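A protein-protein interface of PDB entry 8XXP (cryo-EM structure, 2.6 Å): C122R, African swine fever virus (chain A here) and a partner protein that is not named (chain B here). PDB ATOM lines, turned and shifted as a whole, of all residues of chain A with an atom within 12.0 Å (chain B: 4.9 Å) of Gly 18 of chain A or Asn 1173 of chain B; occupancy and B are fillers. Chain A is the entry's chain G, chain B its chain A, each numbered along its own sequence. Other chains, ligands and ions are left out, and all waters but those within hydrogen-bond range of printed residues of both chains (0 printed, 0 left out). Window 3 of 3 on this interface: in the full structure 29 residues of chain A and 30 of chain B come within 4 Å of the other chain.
Of the printed residues of chain B, Tyr 15 of chain A touches Tyr 1133.
Gly 18 of chain A touches two residues of chain B.
Ile 20 of chain A touches none of the printed residues of chain B.
Of the printed residues of chain B, Leu 38 of chain A touches Leu 1132 (3.5 Å).
Of the printed residues of chain B, Val 39 of chain A touches Tyr 1133 and Trp 1174.
Of chain A, only Tyr 15, Asp 17, Gly 18, Leu 37 and Val 39 come within 4 Å of Tyr 1133 of chain B.
No residue of chain A comes within 4 Å of Glu 1134 of chain B.
No residue of chain A comes within 4 Å of Thr 1135 of chain B.
No residue of chain A comes within 4 Å of Ile 1171 of chain B.
No residue of chain A comes within 4 Å of Ala 1172 of chain B.
No residue of chain A comes within 4 Å of Cys 1175 of chain B.
The nearest residue of chain A that does not touch Asn 1173 of chain B is Asn 19 of chain A (5.1 Å).
The nearest printed residue of chain B that does not touch Asp 17 of chain A is Trp 1174 of chain B (6.5 Å).
Of the 9 printed residues of chain B, 4 touch a printed residue of chain A.
Hydrophobic or aromatic side chains of chain A within 4 Å of the printed part of chain B: Tyr 15, Leu 37, Leu 38 and Val 39.
Among the printed residues, 10 pairs touch across the chains.
Among the printed residues, no Asp or Glu carboxylate lies within 4 Å of a Lys or Arg side-chain nitrogen of the other chain.
Tyr 15 of chain A touches Tyr 1133 of chain B.
Gly 18 of chain A touches Tyr 1133 of chain B.
CA of Gly 18 of chain A touches ND2 of Asn 1173 of chain B, at 3.7 Å.
Leu 1132 of chain B touches Leu 37 of chain A.
Leu 38 of chain A touches Leu 1132 of chain B.
Tyr 1133 of chain B touches Val 39 of chain A (CB to CG2, 3.9 Å).
Trp 1174 of chain B touches Val 39 of chain A.
The side-chain hydroxyl (OH) of Tyr 1133 of chain B is in hydrogen-bond range of the side-chain amide nitrogen (ND2) of Asn 1173 of chain B (2.9 Å).
The backbone carbonyl oxygen of Cys 1175 of chain B sits at hydrogen-bond distance from the backbone NH of Leu 1132 of chain B.
N of Glu 1134 of chain B sits at hydrogen-bond distance from O of Asn 1173 of chain B (2.7 Å).
O of Asn 36 of chain A lies within hydrogen-bond range of OH of Tyr 15 of chain A (2.8 Å).
The guanidinium group (NH2) of Arg 13 of chain A lies within hydrogen-bond range of the side-chain hydroxyl (OH) of Tyr 15 of chain A (2.7 Å).
The guanidinium group (NH2) of Arg 13 of chain A lies within hydrogen-bond range of the backbone carbonyl oxygen (O) of Leu 38 of chain A (3.3 Å).
The side-chain amide nitrogen of Asn 1173 of chain B is in hydrogen-bond range of the backbone carbonyl oxygen of Asp 17 of chain A.
N of Tyr 1133 of chain B lies within hydrogen-bond range of O of Leu 37 of chain A, 2.7 Å away.
O of Asp 17 of chain A sits close to OH of Tyr 1133 of chain B (2.3 Å).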
ATOM      1  N   ARG A  13      14.477  -1.893   8.185  1.00  0.00           N
ATOM      2  CA  ARG A  13      14.446  -1.507   9.594  1.00  0.00           C
ATOM      3  C   ARG A  13      15.849  -1.268  10.145  1.00  0.00           C
ATOM      4  O   ARG A  13      16.179  -0.153  10.561  1.00  0.00           O
ATOM      5  CB  ARG A  13      13.717  -2.572  10.416  1.00  0.00           C
ATOM      6  CG  ARG A  13      12.327  -2.918   9.912  1.00  0.00           C
ATOM      7  CD  ARG A  13      11.589  -3.818  10.894  1.00  0.00           C
ATOM      8  NE  ARG A  13      10.953  -3.066  11.968  1.00  0.00           N
ATOM      9  CZ  ARG A  13       9.716  -2.597  11.923  1.00  0.00           C
ATOM     10  NH1 ARG A  13       8.941  -2.793  10.871  1.00  0.00           N
ATOM     11  NH2 ARG A  13       9.243  -1.911  12.959  1.00  0.00           N
ATOM     12  N   THR A  14      16.688  -2.302  10.158  1.00  0.00           N
ATOM     13  CA  THR A  14      18.039  -2.217  10.719  1.00  0.00           C
ATOM     14  C   THR A  14      18.012  -1.665  12.146  1.00  0.00           C
ATOM     15  O   THR A  14      18.454  -0.553  12.422  1.00  0.00           O
ATOM     16  CB  THR A  14      18.970  -1.365   9.850  1.00  0.00           C
ATOM     17  OG1 THR A  14      18.644   0.020  10.013  1.00  0.00           O
ATOM     18  CG2 THR A  14      18.861  -1.753   8.399  1.00  0.00           C
ATOM     19  N   TYR A  15      17.458  -2.471  13.049  1.00  0.00           N
ATOM     20  CA  TYR A  15      17.423  -2.092  14.456  1.00  0.00           C
ATOM     21  C   TYR A  15      18.836  -1.957  15.004  1.00  0.00           C
ATOM     22  O   TYR A  15      19.504  -2.963  15.273  1.00  0.00           O
ATOM     23  CB  TYR A  15      16.645  -3.128  15.264  1.00  0.00           C
ATOM     24  CG  TYR A  15      15.154  -2.970  15.172  1.00  0.00           C
ATOM     25  CD1 TYR A  15      14.494  -2.015  15.927  1.00  0.00           C
ATOM     26  CD2 TYR A  15      14.408  -3.757  14.319  1.00  0.00           C
ATOM     27  CE1 TYR A  15      13.128  -1.859  15.843  1.00  0.00           C
ATOM     28  CE2 TYR A  15      13.043  -3.609  14.228  1.00  0.00           C
ATOM     29  CZ  TYR A  15      12.407  -2.657  14.990  1.00  0.00           C
ATOM     30  OH  TYR A  15      11.044  -2.511  14.898  1.00  0.00           O
ATOM     31  N   VAL A  16      19.295  -0.719  15.179  1.00  0.00           N
ATOM     32  CA  VAL A  16      20.639  -0.426  15.668  1.00  0.00           C
ATOM     33  C   VAL A  16      20.562   0.845  16.502  1.00  0.00           C
ATOM     34  O   VAL A  16      20.266   1.921  15.972  1.00  0.00           O
ATOM     35  CB  VAL A  16      21.664  -0.260  14.532  1.00  0.00           C
ATOM     36  CG1 VAL A  16      22.935   0.395  15.056  1.00  0.00           C
ATOM     37  CG2 VAL A  16      21.997  -1.607  13.904  1.00  0.00           C
ATOM     38  N   ASP A  17      20.802   0.722  17.803  1.00  0.00           N
ATOM     39  CA  ASP A  17      20.944  -0.548  18.504  1.00  0.00           C
ATOM     40  C   ASP A  17      19.945  -0.533  19.648  1.00  0.00           C
ATOM     41  O   ASP A  17      19.369  -1.557  20.007  1.00  0.00           O
ATOM     42  CB  ASP A  17      22.371  -0.762  19.014  1.00  0.00           C
ATOM     43  CG  ASP A  17      22.899   0.426  19.789  1.00  0.00           C
ATOM     44  OD1 ASP A  17      22.195   1.454  19.867  1.00  0.00           O
ATOM     45  OD2 ASP A  17      24.019   0.328  20.327  1.00  0.00           O
ATOM     46  N   GLY A  18      19.754   0.654  20.212  1.00  0.00           N
ATOM     47  CA  GLY A  18      18.652   0.937  21.100  1.00  0.00           C
ATOM     48  C   GLY A  18      17.502   1.648  20.430  1.00  0.00           C
ATOM     49  O   GLY A  18      16.482   1.905  21.077  1.00  0.00           O
ATOM     50  N   ASN A  19      17.631   1.971  19.145  1.00  0.00           N
ATOM     51  CA  ASN A  19      16.601   2.687  18.412  1.00  0.00           C
ATOM     52  C   ASN A  19      16.495   2.116  17.006  1.00  0.00           C
ATOM     53  O   ASN A  19      17.419   1.476  16.499  1.00  0.00           O
ATOM     54  CB  ASN A  19      16.895   4.193  18.357  1.00  0.00           C
ATOM     55  CG  ASN A  19      16.303   4.944  19.532  1.00  0.00           C
ATOM     56  OD1 ASN A  19      15.261   4.566  20.065  1.00  0.00           O
ATOM     57  ND2 ASN A  19      16.970   6.015  19.947  1.00  0.00           N
ATOM     58  N   ILE A  20      15.343   2.338  16.390  1.00  0.00           N
ATOM     59  CA  ILE A  20      15.140   2.010  14.983  1.00  0.00           C
ATOM     60  C   ILE A  20      15.683   3.122  14.098  1.00  0.00           C
ATOM     61  O   ILE A  20      15.545   4.314  14.397  1.00  0.00           O
ATOM     62  CB  ILE A  20      13.655   1.728  14.694  1.00  0.00           C
ATOM     63  CG1 ILE A  20      13.502   0.952  13.383  1.00  0.00           C
ATOM     64  CG2 ILE A  20      12.847   3.000  14.687  1.00  0.00           C
ATOM     65  CD1 ILE A  20      14.483  -0.151  13.194  1.00  0.00           C
ATOM     66  N   ILE A  21      16.326   2.721  13.008  1.00  0.00           N
ATOM     67  CA  ILE A  21      16.875   3.673  12.057  1.00  0.00           C
ATOM     68  C   ILE A  21      16.588   3.164  10.651  1.00  0.00           C
ATOM     69  O   ILE A  21      17.272   2.268  10.146  1.00  0.00           O
ATOM     70  CB  ILE A  21      18.379   3.896  12.307  1.00  0.00           C
ATOM     71  CG1 ILE A  21      19.014   4.664  11.151  1.00  0.00           C
ATOM     72  CG2 ILE A  21      19.091   2.578  12.595  1.00  0.00           C
ATOM     73  CD1 ILE A  21      18.662   6.123  11.165  1.00  0.00           C
ATOM     74  N   PHE A  22      15.560   3.721  10.016  1.00  0.00           N
ATOM     75  CA  PHE A  22      15.165   3.271   8.688  1.00  0.00           C
ATOM     76  C   PHE A  22      16.244   3.602   7.670  1.00  0.00           C
ATOM     77  O   PHE A  22      16.744   4.728   7.627  1.00  0.00           O
ATOM     78  CB  PHE A  22      13.841   3.911   8.286  1.00  0.00           C
ATOM     79  CG  PHE A  22      12.648   3.241   8.884  1.00  0.00           C
ATOM     80  CD1 PHE A  22      12.257   1.985   8.453  1.00  0.00           C
ATOM     81  CD2 PHE A  22      11.922   3.856   9.885  1.00  0.00           C
ATOM     82  CE1 PHE A  22      11.161   1.360   9.003  1.00  0.00           C
ATOM     83  CE2 PHE A  22      10.825   3.235  10.439  1.00  0.00           C
ATOM     84  CZ  PHE A  22      10.444   1.985   9.998  1.00  0.00           C
ATOM     85  N   GLN A  31      15.443   7.404  11.066  1.00  0.00           N
ATOM     86  CA  GLN A  31      15.400   6.912  12.448  1.00  0.00           C
ATOM     87  C   GLN A  31      14.018   6.317  12.695  1.00  0.00           C
ATOM     88  O   GLN A  31      13.638   5.378  11.975  1.00  0.00           O
ATOM     89  CB  GLN A  31      15.824   8.035  13.395  1.00  0.00           C
ATOM     90  CG  GLN A  31      16.278   7.561  14.763  1.00  0.00           C
ATOM     91  CD  GLN A  31      16.722   8.704  15.647  1.00  0.00           C
ATOM     92  OE1 GLN A  31      17.018   9.795  15.164  1.00  0.00           O
ATOM     93  NE2 GLN A  31      16.759   8.464  16.951  1.00  0.00           N
ATOM     94  N   GLY A  32      13.252   6.794  13.673  1.00  0.00           N
ATOM     95  CA  GLY A  32      11.928   6.257  13.919  1.00  0.00           C
ATOM     96  C   GLY A  32      11.385   6.601  15.289  1.00  0.00           C
ATOM     97  O   GLY A  32      12.147   6.747  16.248  1.00  0.00           O
ATOM     98  N   ASP A  33      10.065   6.724  15.395  1.00  0.00           N
ATOM     99  CA  ASP A  33       9.423   7.141  16.631  1.00  0.00           C
ATOM    100  C   ASP A  33       9.100   5.923  17.493  1.00  0.00           C
ATOM    101  O   ASP A  33       9.562   4.808  17.237  1.00  0.00           O
ATOM    102  CB  ASP A  33       8.178   7.968  16.323  1.00  0.00           C
ATOM    103  CG  ASP A  33       8.511   9.316  15.714  1.00  0.00           C
ATOM    104  OD1 ASP A  33       9.510   9.934  16.140  1.00  0.00           O
ATOM    105  OD2 ASP A  33       7.777   9.758  14.805  1.00  0.00           O
ATOM    106  N   SER A  34       8.304   6.134  18.544  1.00  0.00           N
ATOM    107  CA  SER A  34       7.987   5.047  19.465  1.00  0.00           C
ATOM    108  C   SER A  34       7.087   4.002  18.822  1.00  0.00           C
ATOM    109  O   SER A  34       7.030   2.862  19.297  1.00  0.00           O
ATOM    110  CB  SER A  34       7.330   5.601  20.726  1.00  0.00           C
ATOM    111  OG  SER A  34       6.090   6.215  20.424  1.00  0.00           O
ATOM    112  N   GLN A  35       6.377   4.365  17.754  1.00  0.00           N
ATOM    113  CA  GLN A  35       5.474   3.420  17.112  1.00  0.00           C
ATOM    114  C   GLN A  35       6.195   2.463  16.171  1.00  0.00           C
ATOM    115  O   GLN A  35       5.573   1.511  15.692  1.00  0.00           O
ATOM    116  CB  GLN A  35       4.376   4.181  16.366  1.00  0.00           C
ATOM    117  CG  GLN A  35       3.383   4.854  17.301  1.00  0.00           C
ATOM    118  CD  GLN A  35       2.078   5.237  16.623  1.00  0.00           C
ATOM    119  OE1 GLN A  35       2.021   5.427  15.407  1.00  0.00           O
ATOM    120  NE2 GLN A  35       1.019   5.355  17.414  1.00  0.00           N
ATOM    121  N   ASN A  36       7.480   2.676  15.913  1.00  0.00           N
ATOM    122  CA  ASN A  36       8.242   1.824  15.011  1.00  0.00           C
ATOM    123  C   ASN A  36       8.852   0.615  15.708  1.00  0.00           C
ATOM    124  O   ASN A  36       9.574  -0.152  15.062  1.00  0.00           O
ATOM    125  CB  ASN A  36       9.354   2.631  14.335  1.00  0.00           C
ATOM    126  CG  ASN A  36       8.830   3.582  13.276  1.00  0.00           C
ATOM    127  OD1 ASN A  36       8.993   4.795  13.383  1.00  0.00           O
ATOM    128  ND2 ASN A  36       8.203   3.031  12.243  1.00  0.00           N
ATOM    129  N   LEU A  37       8.586   0.426  16.999  1.00  0.00           N
ATOM    130  CA  LEU A  37       9.204  -0.650  17.765  1.00  0.00           C
ATOM    131  C   LEU A  37       8.476  -1.983  17.640  1.00  0.00           C
ATOM    132  O   LEU A  37       8.931  -2.968  18.227  1.00  0.00           O
ATOM    133  CB  LEU A  37       9.295  -0.254  19.239  1.00  0.00           C
ATOM    134  CG  LEU A  37      10.105   1.009  19.540  1.00  0.00           C
ATOM    135  CD1 LEU A  37      10.073   1.327  21.022  1.00  0.00           C
ATOM    136  CD2 LEU A  37      11.535   0.860  19.054  1.00  0.00           C
ATOM    137  N   LEU A  38       7.367  -2.045  16.908  1.00  0.00           N
ATOM    138  CA  LEU A  38       6.622  -3.291  16.735  1.00  0.00           C
ATOM    139  C   LEU A  38       7.299  -4.100  15.635  1.00  0.00           C
ATOM    140  O   LEU A  38       7.023  -3.910  14.450  1.00  0.00           O
ATOM    141  CB  LEU A  38       5.165  -2.997  16.399  1.00  0.00           C
ATOM    142  CG  LEU A  38       4.099  -4.078  16.588  1.00  0.00           C
ATOM    143  CD1 LEU A  38       4.108  -5.089  15.454  1.00  0.00           C
ATOM    144  CD2 LEU A  38       4.281  -4.768  17.916  1.00  0.00           C
ATOM    145  N   VAL A  39       8.189  -5.010  16.025  1.00  0.00           N
ATOM    146  CA  VAL A  39       8.952  -5.771  15.043  1.00  0.00           C
ATOM    147  C   VAL A  39       8.084  -6.823  14.367  1.00  0.00           C
ATOM    148  O   VAL A  39       8.151  -7.008  13.147  1.00  0.00           O
ATOM    149  CB  VAL A  39      10.180  -6.401  15.712  1.00  0.00           C
ATOM    150  CG1 VAL A  39      11.089  -7.010  14.670  1.00  0.00           C
ATOM    151  CG2 VAL A  39      10.910  -5.360  16.528  1.00  0.00           C
ATOM    152  N   SER A  40       7.271  -7.535  15.141  1.00  0.00           N
ATOM    153  CA  SER A  40       6.369  -8.540  14.604  1.00  0.00           C
ATOM    154  C   SER A  40       5.193  -8.689  15.553  1.00  0.00           C
ATOM    155  O   SER A  40       5.205  -8.173  16.673  1.00  0.00           O
ATOM    156  CB  SER A  40       7.072  -9.885  14.395  1.00  0.00           C
ATOM    157  OG  SER A  40       7.829  -9.877  13.199  1.00  0.00           O
ATOM    158  N   LEU B1132       8.271  -6.828  20.506  1.00  0.00           N
ATOM    159  CA  LEU B1132       8.572  -5.409  20.597  1.00  0.00           C
ATOM    160  C   LEU B1132      10.076  -5.182  20.599  1.00  0.00           C
ATOM    161  O   LEU B1132      10.865  -6.082  20.890  1.00  0.00           O
ATOM    162  CB  LEU B1132       7.960  -4.805  21.861  1.00  0.00           C
ATOM    163  CG  LEU B1132       6.483  -5.087  22.104  1.00  0.00           C
ATOM    164  CD1 LEU B1132       6.104  -4.758  23.533  1.00  0.00           C
ATOM    165  CD2 LEU B1132       5.656  -4.275  21.149  1.00  0.00           C
ATOM    166  N   TYR B1133      10.467  -3.963  20.234  1.00  0.00           N
ATOM    167  CA  TYR B1133      11.848  -3.514  20.387  1.00  0.00           C
ATOM    168  C   TYR B1133      11.913  -2.541  21.556  1.00  0.00           C
ATOM    169  O   TYR B1133      11.914  -1.323  21.390  1.00  0.00           O
ATOM    170  CB  TYR B1133      12.356  -2.879  19.107  1.00  0.00           C
ATOM    171  CG  TYR B1133      13.857  -2.877  19.005  1.00  0.00           C
ATOM    172  CD1 TYR B1133      14.550  -4.042  18.712  1.00  0.00           C
ATOM    173  CD2 TYR B1133      14.583  -1.710  19.196  1.00  0.00           C
ATOM    174  CE1 TYR B1133      15.921  -4.046  18.613  1.00  0.00           C
ATOM    175  CE2 TYR B1133      15.952  -1.702  19.089  1.00  0.00           C
ATOM    176  CZ  TYR B1133      16.617  -2.875  18.797  1.00  0.00           C
ATOM    177  OH  TYR B1133      17.989  -2.879  18.701  1.00  0.00           O
ATOM    178  N   GLU B1134      11.990  -3.094  22.759  1.00  0.00           N
ATOM    179  CA  GLU B1134      12.092  -2.255  23.939  1.00  0.00           C
ATOM    180  C   GLU B1134      12.700  -3.066  25.069  1.00  0.00           C
ATOM    181  O   GLU B1134      12.566  -4.289  25.115  1.00  0.00           O
ATOM    182  CB  GLU B1134      10.727  -1.689  24.339  1.00  0.00           C
ATOM    183  CG  GLU B1134       9.644  -2.731  24.501  1.00  0.00           C
ATOM    184  CD  GLU B1134       8.296  -2.108  24.772  1.00  0.00           C
ATOM    185  OE1 GLU B1134       7.997  -1.065  24.159  1.00  0.00           O
ATOM    186  OE2 GLU B1134       7.536  -2.659  25.593  1.00  0.00           O
ATOM    187  N   THR B1135      13.373  -2.362  25.975  1.00  0.00           N
ATOM    188  CA  THR B1135      14.075  -2.975  27.089  1.00  0.00           C
ATOM    189  C   THR B1135      13.504  -2.443  28.393  1.00  0.00           C
ATOM    190  O   THR B1135      12.780  -1.447  28.417  1.00  0.00           O
ATOM    191  CB  THR B1135      15.585  -2.705  27.024  1.00  0.00           C
ATOM    192  OG1 THR B1135      16.290  -3.760  27.688  1.00  0.00           O
ATOM    193  CG2 THR B1135      15.929  -1.376  27.674  1.00  0.00           C
ATOM    194  N   ILE B1171      20.411  -7.866  29.999  1.00  0.00           N
ATOM    195  CA  ILE B1171      19.156  -7.898  29.265  1.00  0.00           C
ATOM    196  C   ILE B1171      19.350  -7.291  27.881  1.00  0.00           C
ATOM    197  O   ILE B1171      20.286  -6.518  27.636  1.00  0.00           O
ATOM    198  CB  ILE B1171      18.064  -7.152  30.055  1.00  0.00           C
ATOM    199  CG1 ILE B1171      16.703  -7.817  29.874  1.00  0.00           C
ATOM    200  CG2 ILE B1171      17.988  -5.696  29.637  1.00  0.00           C
ATOM    201  CD1 ILE B1171      15.594  -7.103  30.610  1.00  0.00           C
ATOM    202  N   ALA B1172      18.473  -7.661  26.958  1.00  0.00           N
ATOM    203  CA  ALA B1172      18.419  -7.057  25.639  1.00  0.00           C
ATOM    204  C   ALA B1172      17.177  -6.183  25.532  1.00  0.00           C
ATOM    205  O   ALA B1172      16.338  -6.128  26.435  1.00  0.00           O
ATOM    206  CB  ALA B1172      18.437  -8.125  24.546  1.00  0.00           C
ATOM    207  N   ASN B1173      17.071  -5.482  24.407  1.00  0.00           N
ATOM    208  CA  ASN B1173      15.924  -4.638  24.107  1.00  0.00           C
ATOM    209  C   ASN B1173      14.929  -5.331  23.189  1.00  0.00           C
ATOM    210  O   ASN B1173      14.150  -4.671  22.497  1.00  0.00           O
ATOM    211  CB  ASN B1173      16.402  -3.315  23.518  1.00  0.00           C
ATOM    212  CG  ASN B1173      17.478  -3.505  22.480  1.00  0.00           C
ATOM    213  OD1 ASN B1173      18.279  -4.436  22.562  1.00  0.00           O
ATOM    214  ND2 ASN B1173      17.552  -2.585  21.540  1.00  0.00           N
ATOM    215  N   TRP B1174      14.946  -6.659  23.177  1.00  0.00           N
ATOM    216  CA  TRP B1174      14.000  -7.473  22.428  1.00  0.00           C
ATOM    217  C   TRP B1174      12.987  -8.021  23.422  1.00  0.00           C
ATOM    218  O   TRP B1174      13.324  -8.873  24.248  1.00  0.00           O
ATOM    219  CB  TRP B1174      14.716  -8.606  21.699  1.00  0.00           C
ATOM    220  CG  TRP B1174      15.480  -8.166  20.499  1.00  0.00           C
ATOM    221  CD1 TRP B1174      16.822  -7.961  20.416  1.00  0.00           C
ATOM    222  CD2 TRP B1174      14.949  -7.878  19.202  1.00  0.00           C
ATOM    223  NE1 TRP B1174      17.165  -7.567  19.147  1.00  0.00           N
ATOM    224  CE2 TRP B1174      16.031  -7.506  18.382  1.00  0.00           C
ATOM    225  CE3 TRP B1174      13.663  -7.898  18.654  1.00  0.00           C
ATOM    226  CZ2 TRP B1174      15.869  -7.158  17.047  1.00  0.00           C
ATOM    227  CZ3 TRP B1174      13.504  -7.553  17.333  1.00  0.00           C
ATOM    228  CH2 TRP B1174      14.600  -7.186  16.544  1.00  0.00           C
ATOM    229  N   CYS B1175      11.754  -7.534  23.343  1.00  0.00           N
ATOM    230  CA  CYS B1175      10.687  -7.950  24.236  1.00  0.00           C
ATOM    231  C   CYS B1175       9.620  -8.695  23.448  1.00  0.00           C
ATOM    232  O   CYS B1175       9.371  -8.397  22.277  1.00  0.00           O
ATOM    233  CB  CYS B1175      10.065  -6.749  24.947  1.00  0.00           C
ATOM    234  SG  CYS B1175       8.632  -7.135  25.963  1.00  0.00           S
